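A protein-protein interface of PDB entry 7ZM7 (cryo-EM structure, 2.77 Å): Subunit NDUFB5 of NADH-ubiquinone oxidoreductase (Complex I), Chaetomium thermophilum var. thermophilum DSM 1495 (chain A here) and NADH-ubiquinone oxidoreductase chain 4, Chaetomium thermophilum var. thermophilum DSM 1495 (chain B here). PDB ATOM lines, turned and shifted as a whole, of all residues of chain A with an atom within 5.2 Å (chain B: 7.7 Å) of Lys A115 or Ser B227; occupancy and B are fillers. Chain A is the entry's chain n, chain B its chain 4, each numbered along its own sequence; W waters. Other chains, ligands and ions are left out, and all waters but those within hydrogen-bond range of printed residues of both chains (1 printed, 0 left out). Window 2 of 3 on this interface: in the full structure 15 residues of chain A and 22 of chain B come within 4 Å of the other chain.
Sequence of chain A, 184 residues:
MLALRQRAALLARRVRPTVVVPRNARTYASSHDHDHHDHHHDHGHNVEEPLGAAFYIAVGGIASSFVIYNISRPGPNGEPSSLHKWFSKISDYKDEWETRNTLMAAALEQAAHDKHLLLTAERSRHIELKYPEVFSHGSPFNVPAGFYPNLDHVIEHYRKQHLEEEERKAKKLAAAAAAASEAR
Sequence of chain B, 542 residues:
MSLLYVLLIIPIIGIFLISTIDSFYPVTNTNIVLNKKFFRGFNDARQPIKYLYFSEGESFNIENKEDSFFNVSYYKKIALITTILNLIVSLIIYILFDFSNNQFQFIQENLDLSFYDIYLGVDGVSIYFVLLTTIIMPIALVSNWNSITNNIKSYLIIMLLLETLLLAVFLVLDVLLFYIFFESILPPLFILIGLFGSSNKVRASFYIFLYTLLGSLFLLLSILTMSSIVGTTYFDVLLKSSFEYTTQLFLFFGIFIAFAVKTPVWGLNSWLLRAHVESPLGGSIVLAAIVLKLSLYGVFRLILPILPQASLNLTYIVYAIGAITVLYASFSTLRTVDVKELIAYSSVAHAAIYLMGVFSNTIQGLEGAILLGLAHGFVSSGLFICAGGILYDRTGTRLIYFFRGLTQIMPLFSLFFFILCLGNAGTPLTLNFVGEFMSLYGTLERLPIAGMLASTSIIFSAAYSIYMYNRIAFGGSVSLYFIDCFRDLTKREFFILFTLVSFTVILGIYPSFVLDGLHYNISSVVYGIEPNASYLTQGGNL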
ATOM      1  N   ALA A 111       9.172   8.679  -4.595  1.00  0.00           N
ATOM      2  CA  ALA A 111       7.927   8.454  -5.305  1.00  0.00           C
ATOM      3  C   ALA A 111       6.744   9.068  -4.578  1.00  0.00           C
ATOM      4  O   ALA A 111       5.679   9.241  -5.172  1.00  0.00           O
ATOM      5  CB  ALA A 111       7.714   6.964  -5.522  1.00  0.00           C
ATOM      6  N   ALA A 112       6.888   9.365  -3.292  1.00  0.00           N
ATOM      7  CA  ALA A 112       5.900  10.206  -2.630  1.00  0.00           C
ATOM      8  C   ALA A 112       5.876  11.592  -3.255  1.00  0.00           C
ATOM      9  O   ALA A 112       4.808  12.171  -3.469  1.00  0.00           O
ATOM     10  CB  ALA A 112       6.198  10.296  -1.139  1.00  0.00           C
ATOM     11  N   HIS A 113       7.055  12.117  -3.595  1.00  0.00           N
ATOM     12  CA  HIS A 113       7.137  13.452  -4.236  1.00  0.00           C
ATOM     13  C   HIS A 113       6.652  13.355  -5.680  1.00  0.00           C
ATOM     14  O   HIS A 113       5.934  14.281  -6.119  1.00  0.00           O
ATOM     15  CB  HIS A 113       8.574  13.988  -4.177  1.00  0.00           C
ATOM     16  CG  HIS A 113       8.923  14.883  -5.316  1.00  0.00           C
ATOM     17  ND1 HIS A 113       8.473  16.184  -5.398  1.00  0.00           N
ATOM     18  CD2 HIS A 113       9.667  14.668  -6.423  1.00  0.00           C
ATOM     19  CE1 HIS A 113       8.925  16.732  -6.508  1.00  0.00           C
ATOM     20  NE2 HIS A 113       9.660  15.823  -7.155  1.00  0.00           N
ATOM     21  N   ASP A 114       7.010  12.281  -6.388  1.00  0.00           N
ATOM     22  CA  ASP A 114       6.678  12.183  -7.802  1.00  0.00           C
ATOM     23  C   ASP A 114       5.198  11.985  -8.046  1.00  0.00           C
ATOM     24  O   ASP A 114       4.697  12.408  -9.088  1.00  0.00           O
ATOM     25  CB  ASP A 114       7.440  11.038  -8.449  1.00  0.00           C
ATOM     26  CG  ASP A 114       8.741  11.479  -9.044  1.00  0.00           C
ATOM     27  OD1 ASP A 114       9.047  12.683  -8.974  1.00  0.00           O
ATOM     28  OD2 ASP A 114       9.457  10.622  -9.594  1.00  0.00           O
ATOM     29  N   LYS A 115       4.499  11.341  -7.118  1.00  0.00           N
ATOM     30  CA  LYS A 115       3.073  11.123  -7.281  1.00  0.00           C
ATOM     31  C   LYS A 115       2.291  12.398  -7.008  1.00  0.00           C
ATOM     32  O   LYS A 115       1.280  12.658  -7.665  1.00  0.00           O
ATOM     33  CB  LYS A 115       2.629   9.981  -6.371  1.00  0.00           C
ATOM     34  CG  LYS A 115       1.206  10.031  -5.934  1.00  0.00           C
ATOM     35  CD  LYS A 115       0.989   9.091  -4.790  1.00  0.00           C
ATOM     36  CE  LYS A 115      -0.343   9.329  -4.120  1.00  0.00           C
ATOM     37  NZ  LYS A 115      -0.580   8.327  -3.049  1.00  0.00           N
ATOM     38  N   HIS A 116       2.745  13.214  -6.056  1.00  0.00           N
ATOM     39  CA  HIS A 116       2.189  14.555  -5.913  1.00  0.00           C
ATOM     40  C   HIS A 116       2.378  15.377  -7.178  1.00  0.00           C
ATOM     41  O   HIS A 116       1.475  16.102  -7.592  1.00  0.00           O
ATOM     42  CB  HIS A 116       2.821  15.276  -4.726  1.00  0.00           C
ATOM     43  CG  HIS A 116       2.281  14.868  -3.396  1.00  0.00           C
ATOM     44  ND1 HIS A 116       2.855  15.266  -2.213  1.00  0.00           N
ATOM     45  CD2 HIS A 116       1.184  14.158  -3.059  1.00  0.00           C
ATOM     46  CE1 HIS A 116       2.151  14.794  -1.203  1.00  0.00           C
ATOM     47  NE2 HIS A 116       1.130  14.119  -1.690  1.00  0.00           N
ATOM     48  N   LEU A 117       3.560  15.353  -7.774  1.00  0.00           N
ATOM     49  CA  LEU A 117       3.853  16.172  -8.980  1.00  0.00           C
ATOM     50  C   LEU A 117       2.937  15.757 -10.130  1.00  0.00           C
ATOM     51  O   LEU A 117       2.353  16.634 -10.762  1.00  0.00           O
ATOM     52  CB  LEU A 117       5.320  15.947  -9.343  1.00  0.00           C
ATOM     53  CG  LEU A 117       5.839  16.704 -10.560  1.00  0.00           C
ATOM     54  CD1 LEU A 117       6.009  18.180 -10.242  1.00  0.00           C
ATOM     55  CD2 LEU A 117       7.154  16.105 -11.018  1.00  0.00           C
ATOM     56  N   LEU A 118       2.771  14.496 -10.390  1.00  0.00           N
ATOM     57  CA  LEU A 118       1.962  14.032 -11.539  1.00  0.00           C
ATOM     58  C   LEU A 118       0.467  14.200 -11.259  1.00  0.00           C
ATOM     59  O   LEU A 118      -0.262  14.510 -12.203  1.00  0.00           O
ATOM     60  CB  LEU A 118       2.321  12.581 -11.851  1.00  0.00           C
ATOM     61  CG  LEU A 118       3.674  12.341 -12.513  1.00  0.00           C
ATOM     62  CD1 LEU A 118       4.158  10.929 -12.231  1.00  0.00           C
ATOM     63  CD2 LEU A 118       3.595  12.582 -14.009  1.00  0.00           C
ATOM     64  N   LEU A 119       0.050  14.029  -9.990  1.00  0.00           N
ATOM     65  CA  LEU A 119      -1.405  14.089  -9.689  1.00  0.00           C
ATOM     66  C   LEU A 119      -1.889  15.511  -9.401  1.00  0.00           C
ATOM     67  O   LEU A 119      -3.085  15.658  -9.117  1.00  0.00           O
ATOM     68  CB  LEU A 119      -1.688  13.166  -8.497  1.00  0.00           C
ATOM     69  CG  LEU A 119      -2.790  12.129  -8.663  1.00  0.00           C
ATOM     70  CD1 LEU A 119      -2.624  11.365  -9.962  1.00  0.00           C
ATOM     71  CD2 LEU A 119      -2.770  11.174  -7.486  1.00  0.00           C
ATOM     72  N   THR A 120      -0.988  16.490  -9.381  1.00  0.00           N
ATOM     73  CA  THR A 120      -1.375  17.869  -8.977  1.00  0.00           C
ATOM     74  C   THR A 120      -0.950  18.792 -10.107  1.00  0.00           C
ATOM     75  O   THR A 120      -0.600  19.942  -9.813  1.00  0.00           O
ATOM     76  CB  THR A 120      -0.851  18.304  -7.602  1.00  0.00           C
ATOM     77  OG1 THR A 120       0.567  18.444  -7.647  1.00  0.00           O
ATOM     78  CG2 THR A 120      -1.280  17.399  -6.467  1.00  0.00           C
ATOM     79  N   VAL B 175       0.754   0.563   5.313  1.00  0.00           N
ATOM     80  CA  VAL B 175      -0.562   0.509   5.938  1.00  0.00           C
ATOM     81  C   VAL B 175      -1.631   0.186   4.908  1.00  0.00           C
ATOM     82  O   VAL B 175      -2.725  -0.257   5.263  1.00  0.00           O
ATOM     83  CB  VAL B 175      -0.892   1.797   6.726  1.00  0.00           C
ATOM     84  CG1 VAL B 175       0.151   2.070   7.767  1.00  0.00           C
ATOM     85  CG2 VAL B 175      -1.085   2.965   5.834  1.00  0.00           C
ATOM     86  N   LEU B 176      -1.349   0.394   3.624  1.00  0.00           N
ATOM     87  CA  LEU B 176      -2.289  -0.097   2.623  1.00  0.00           C
ATOM     88  C   LEU B 176      -2.082  -1.582   2.380  1.00  0.00           C
ATOM     89  O   LEU B 176      -3.047  -2.330   2.217  1.00  0.00           O
ATOM     90  CB  LEU B 176      -2.184   0.688   1.317  1.00  0.00           C
ATOM     91  CG  LEU B 176      -3.183   0.180   0.275  1.00  0.00           C
ATOM     92  CD1 LEU B 176      -4.518   0.833   0.433  1.00  0.00           C
ATOM     93  CD2 LEU B 176      -2.689   0.365  -1.127  1.00  0.00           C
ATOM     94  N   LEU B 221     -11.040   4.404   4.143  1.00  0.00           N
ATOM     95  CA  LEU B 221     -11.130   5.832   3.859  1.00  0.00           C
ATOM     96  C   LEU B 221     -10.032   6.620   4.567  1.00  0.00           C
ATOM     97  O   LEU B 221      -9.506   7.587   4.014  1.00  0.00           O
ATOM     98  CB  LEU B 221     -12.505   6.363   4.260  1.00  0.00           C
ATOM     99  CG  LEU B 221     -13.767   5.884   3.538  1.00  0.00           C
ATOM    100  CD1 LEU B 221     -14.942   6.615   4.092  1.00  0.00           C
ATOM    101  CD2 LEU B 221     -13.707   6.098   2.044  1.00  0.00           C
ATOM    102  N   SER B 222      -9.684   6.239   5.798  1.00  0.00           N
ATOM    103  CA  SER B 222      -8.648   6.973   6.520  1.00  0.00           C
ATOM    104  C   SER B 222      -7.258   6.652   5.993  1.00  0.00           C
ATOM    105  O   SER B 222      -6.393   7.527   5.954  1.00  0.00           O
ATOM    106  CB  SER B 222      -8.733   6.685   8.019  1.00  0.00           C
ATOM    107  OG  SER B 222      -9.943   7.168   8.540  1.00  0.00           O
ATOM    108  N   ILE B 223      -7.010   5.403   5.616  1.00  0.00           N
ATOM    109  CA  ILE B 223      -5.733   5.050   5.007  1.00  0.00           C
ATOM    110  C   ILE B 223      -5.560   5.804   3.699  1.00  0.00           C
ATOM    111  O   ILE B 223      -4.480   6.305   3.388  1.00  0.00           O
ATOM    112  CB  ILE B 223      -5.638   3.527   4.801  1.00  0.00           C
ATOM    113  CG1 ILE B 223      -5.615   2.802   6.137  1.00  0.00           C
ATOM    114  CG2 ILE B 223      -4.399   3.154   4.017  1.00  0.00           C
ATOM    115  CD1 ILE B 223      -5.711   1.319   6.001  1.00  0.00           C
ATOM    116  N   LEU B 224      -6.639   5.912   2.925  1.00  0.00           N
ATOM    117  CA  LEU B 224      -6.575   6.600   1.648  1.00  0.00           C
ATOM    118  C   LEU B 224      -6.260   8.078   1.830  1.00  0.00           C
ATOM    119  O   LEU B 224      -5.536   8.665   1.027  1.00  0.00           O
ATOM    120  CB  LEU B 224      -7.881   6.399   0.884  1.00  0.00           C
ATOM    121  CG  LEU B 224      -8.139   5.002   0.309  1.00  0.00           C
ATOM    122  CD1 LEU B 224      -9.384   4.968  -0.560  1.00  0.00           C
ATOM    123  CD2 LEU B 224      -6.933   4.470  -0.430  1.00  0.00           C
ATOM    124  N   THR B 225      -6.788   8.692   2.883  1.00  0.00           N
ATOM    125  CA  THR B 225      -6.454  10.078   3.198  1.00  0.00           C
ATOM    126  C   THR B 225      -4.987  10.236   3.580  1.00  0.00           C
ATOM    127  O   THR B 225      -4.313  11.163   3.128  1.00  0.00           O
ATOM    128  CB  THR B 225      -7.347  10.575   4.328  1.00  0.00           C
ATOM    129  OG1 THR B 225      -8.712  10.435   3.935  1.00  0.00           O
ATOM    130  CG2 THR B 225      -7.070  12.025   4.615  1.00  0.00           C
ATOM    131  N   MET B 226      -4.475   9.348   4.421  1.00  0.00           N
ATOM    132  CA  MET B 226      -3.080   9.446   4.826  1.00  0.00           C
ATOM    133  C   MET B 226      -2.151   9.334   3.624  1.00  0.00           C
ATOM    134  O   MET B 226      -1.173  10.078   3.512  1.00  0.00           O
ATOM    135  CB  MET B 226      -2.761   8.346   5.832  1.00  0.00           C
ATOM    136  CG  MET B 226      -3.459   8.489   7.138  1.00  0.00           C
ATOM    137  SD  MET B 226      -3.064   7.168   8.268  1.00  0.00           S
ATOM    138  CE  MET B 226      -4.120   7.587   9.642  1.00  0.00           C
ATOM    139  N   SER B 227      -2.438   8.396   2.722  1.00  0.00           N
ATOM    140  CA  SER B 227      -1.597   8.205   1.551  1.00  0.00           C
ATOM    141  C   SER B 227      -1.621   9.420   0.645  1.00  0.00           C
ATOM    142  O   SER B 227      -0.584   9.823   0.116  1.00  0.00           O
ATOM    143  CB  SER B 227      -2.046   6.974   0.785  1.00  0.00           C
ATOM    144  OG  SER B 227      -1.349   6.860  -0.441  1.00  0.00           O
ATOM    145  N   SER B 228      -2.798  10.008   0.440  1.00  0.00           N
ATOM    146  CA  SER B 228      -2.894  11.171  -0.433  1.00  0.00           C
ATOM    147  C   SER B 228      -2.099  12.346   0.117  1.00  0.00           C
ATOM    148  O   SER B 228      -1.391  13.025  -0.629  1.00  0.00           O
ATOM    149  CB  SER B 228      -4.356  11.558  -0.628  1.00  0.00           C
ATOM    150  OG  SER B 228      -4.855  12.177   0.535  1.00  0.00           O
ATOM    151  N   ILE B 229      -2.189  12.589   1.419  1.00  0.00           N
ATOM    152  CA  ILE B 229      -1.431  13.666   2.045  1.00  0.00           C
ATOM    153  C   ILE B 229       0.066  13.399   1.985  1.00  0.00           C
ATOM    154  O   ILE B 229       0.849  14.290   1.657  1.00  0.00           O
ATOM    155  CB  ILE B 229      -1.911  13.864   3.494  1.00  0.00           C
ATOM    156  CG1 ILE B 229      -3.368  14.325   3.505  1.00  0.00           C
ATOM    157  CG2 ILE B 229      -1.007  14.841   4.232  1.00  0.00           C
ATOM    158  CD1 ILE B 229      -4.054  14.232   4.842  1.00  0.00           C
ATOM    159  N   VAL B 230       0.490  12.179   2.292  1.00  0.00           N
ATOM    160  CA  VAL B 230       1.909  11.883   2.418  1.00  0.00           C
ATOM    161  C   VAL B 230       2.521  11.371   1.112  1.00  0.00           C
ATOM    162  O   VAL B 230       3.709  11.578   0.862  1.00  0.00           O
ATOM    163  CB  VAL B 230       2.125  10.887   3.573  1.00  0.00           C
ATOM    164  CG1 VAL B 230       3.560  10.450   3.660  1.00  0.00           C
ATOM    165  CG2 VAL B 230       1.733  11.497   4.871  1.00  0.00           C
ATOM    166  N   GLY B 231       1.747  10.708   0.270  1.00  0.00           N
ATOM    167  CA  GLY B 231       2.230  10.182  -0.978  1.00  0.00           C
ATOM    168  C   GLY B 231       2.527   8.701  -0.963  1.00  0.00           C
ATOM    169  O   GLY B 231       2.612   8.090  -2.027  1.00  0.00           O
ATOM    170  N   THR B 232       2.682   8.113   0.212  1.00  0.00           N
ATOM    171  CA  THR B 232       2.916   6.688   0.335  1.00  0.00           C
ATOM    172  C   THR B 232       2.341   6.227   1.663  1.00  0.00           C
ATOM    173  O   THR B 232       1.907   7.029   2.489  1.00  0.00           O
ATOM    174  CB  THR B 232       4.418   6.352   0.181  1.00  0.00           C
ATOM    175  OG1 THR B 232       4.618   4.934   0.243  1.00  0.00           O
ATOM    176  CG2 THR B 232       5.268   7.030   1.222  1.00  0.00           C
ATOM    177  N   THR B 233       2.308   4.912   1.841  1.00  0.00           N
ATOM    178  CA  THR B 233       1.917   4.292   3.100  1.00  0.00           C
ATOM    179  C   THR B 233       3.010   3.399   3.659  1.00  0.00           C
ATOM    180  O   THR B 233       2.758   2.666   4.616  1.00  0.00           O
ATOM    181  CB  THR B 233       0.616   3.496   2.942  1.00  0.00           C
ATOM    182  OG1 THR B 233       0.787   2.452   1.977  1.00  0.00           O
ATOM    183  CG2 THR B 233      -0.525   4.388   2.560  1.00  0.00           C
ATOM    184  N   TYR B 234       4.200   3.437   3.069  1.00  0.00           N
ATOM    185  CA  TYR B 234       5.378   2.804   3.638  1.00  0.00           C
ATOM    186  C   TYR B 234       5.668   3.381   5.013  1.00  0.00           C
ATOM    187  O   TYR B 234       5.691   4.598   5.184  1.00  0.00           O
ATOM    188  CB  TYR B 234       6.552   3.035   2.689  1.00  0.00           C
ATOM    189  CG  TYR B 234       7.851   2.382   3.056  1.00  0.00           C
ATOM    190  CD1 TYR B 234       8.025   1.011   2.944  1.00  0.00           C
ATOM    191  CD2 TYR B 234       8.920   3.148   3.477  1.00  0.00           C
ATOM    192  CE1 TYR B 234       9.213   0.433   3.267  1.00  0.00           C
ATOM    193  CE2 TYR B 234      10.098   2.582   3.797  1.00  0.00           C
ATOM    194  CZ  TYR B 234      10.251   1.230   3.693  1.00  0.00           C
ATOM    195  OH  TYR B 234      11.459   0.677   4.020  1.00  0.00           O
ATOM    196  N   LEU B 238       5.637   7.479   6.683  1.00  0.00           N
ATOM    197  CA  LEU B 238       4.534   7.911   7.545  1.00  0.00           C
ATOM    198  C   LEU B 238       4.985   8.339   8.932  1.00  0.00           C
ATOM    199  O   LEU B 238       4.449   9.300   9.486  1.00  0.00           O
ATOM    200  CB  LEU B 238       3.489   6.809   7.682  1.00  0.00           C
ATOM    201  CG  LEU B 238       2.652   6.373   6.501  1.00  0.00           C
ATOM    202  CD1 LEU B 238       1.837   5.193   6.894  1.00  0.00           C
ATOM    203  CD2 LEU B 238       1.704   7.517   6.226  1.00  0.00           C
ATOM    204  N   PHE B 243       0.657  14.704  10.977  1.00  0.00           N
ATOM    205  CA  PHE B 243      -0.607  15.264  10.464  1.00  0.00           C
ATOM    206  C   PHE B 243      -1.093  16.402  11.344  1.00  0.00           C
ATOM    207  O   PHE B 243      -0.737  16.423  12.511  1.00  0.00           O
ATOM    208  CB  PHE B 243      -1.649  14.156  10.357  1.00  0.00           C
ATOM    209  CG  PHE B 243      -1.307  13.061   9.382  1.00  0.00           C
ATOM    210  CD1 PHE B 243      -0.672  11.907   9.807  1.00  0.00           C
ATOM    211  CD2 PHE B 243      -1.627  13.185   8.041  1.00  0.00           C
ATOM    212  CE1 PHE B 243      -0.357  10.902   8.909  1.00  0.00           C
ATOM    213  CE2 PHE B 243      -1.314  12.176   7.144  1.00  0.00           C
ATOM    214  CZ  PHE B 243      -0.679  11.040   7.580  1.00  0.00           C
ATOM    215  N   LEU B 251      -8.857  11.182  11.012  1.00  0.00           N
ATOM    216  CA  LEU B 251      -8.293   9.864  10.776  1.00  0.00           C
ATOM    217  C   LEU B 251      -8.572   8.929  11.944  1.00  0.00           C
ATOM    218  O   LEU B 251      -8.700   7.719  11.750  1.00  0.00           O
ATOM    219  CB  LEU B 251      -6.797   9.988  10.531  1.00  0.00           C
ATOM    220  CG  LEU B 251      -6.458  10.685   9.223  1.00  0.00           C
ATOM    221  CD1 LEU B 251      -5.005  11.078   9.170  1.00  0.00           C
ATOM    222  CD2 LEU B 251      -6.813   9.816   8.067  1.00  0.00           C
HETATM  223  O   HOH W   1      -1.615  13.605  -3.765  1.00  0.00           O
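Val B230 touches Ala A112 (O to CB, 3.4 Å). Gly B231 touches Ala A112 (O to CA, 3.96 Å). Gly B231 touches His A116.
The backbone carbonyl oxygen of Ser B228 lies within hydrogen-bond range of a ring nitrogen (NE2) of His A116 (2.9 Å). The backbone carbonyl oxygen (O) of Gly B231 lies close to the side-chain amino group (NZ) of Lys A115, 3.4 Å away. The backbone carbonyl oxygen (O) of Ile B229 sits close to a ring nitrogen (NE2) of His A116, 3.4 Å away. OG of Ser B227 sits at hydrogen-bond distance from NZ of Lys A115.
The backbone carbonyl oxygen (O) of Thr B225 sits at hydrogen-bond distance from the side-chain hydroxyl (OG) of Ser B228. The side-chain hydroxyl of Thr A120 sits at hydrogen-bond distance from the backbone carbonyl oxygen of His A116, 2.5 Å away.
Asp A114 touches none of the printed residues of chain B. Of chain B, only Ser B227 and Gly B231 come within 4 Å of Lys A115. Printed residues of chain B within 4 Å of His A116: Ser B228, Ile B229 and Gly B231. Ser B227 touches one residue of chain A. Of the printed residues of chain A, Ser B228 touches His A116 (2.9 Å). Leu B238 touches none of the printed residues of chain A. The nearest residue of chain B that does not touch Lys A115 is Ser B228 (4.5 Å).
Water W1 bridges O of Ser B228 (3.2 Å) and NE2 of His A116 (3.5 Å).
Among the printed residues, no Asp or Glu carboxylate lies within 4 Å of a Lys or Arg side-chain nitrogen of the other chain.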
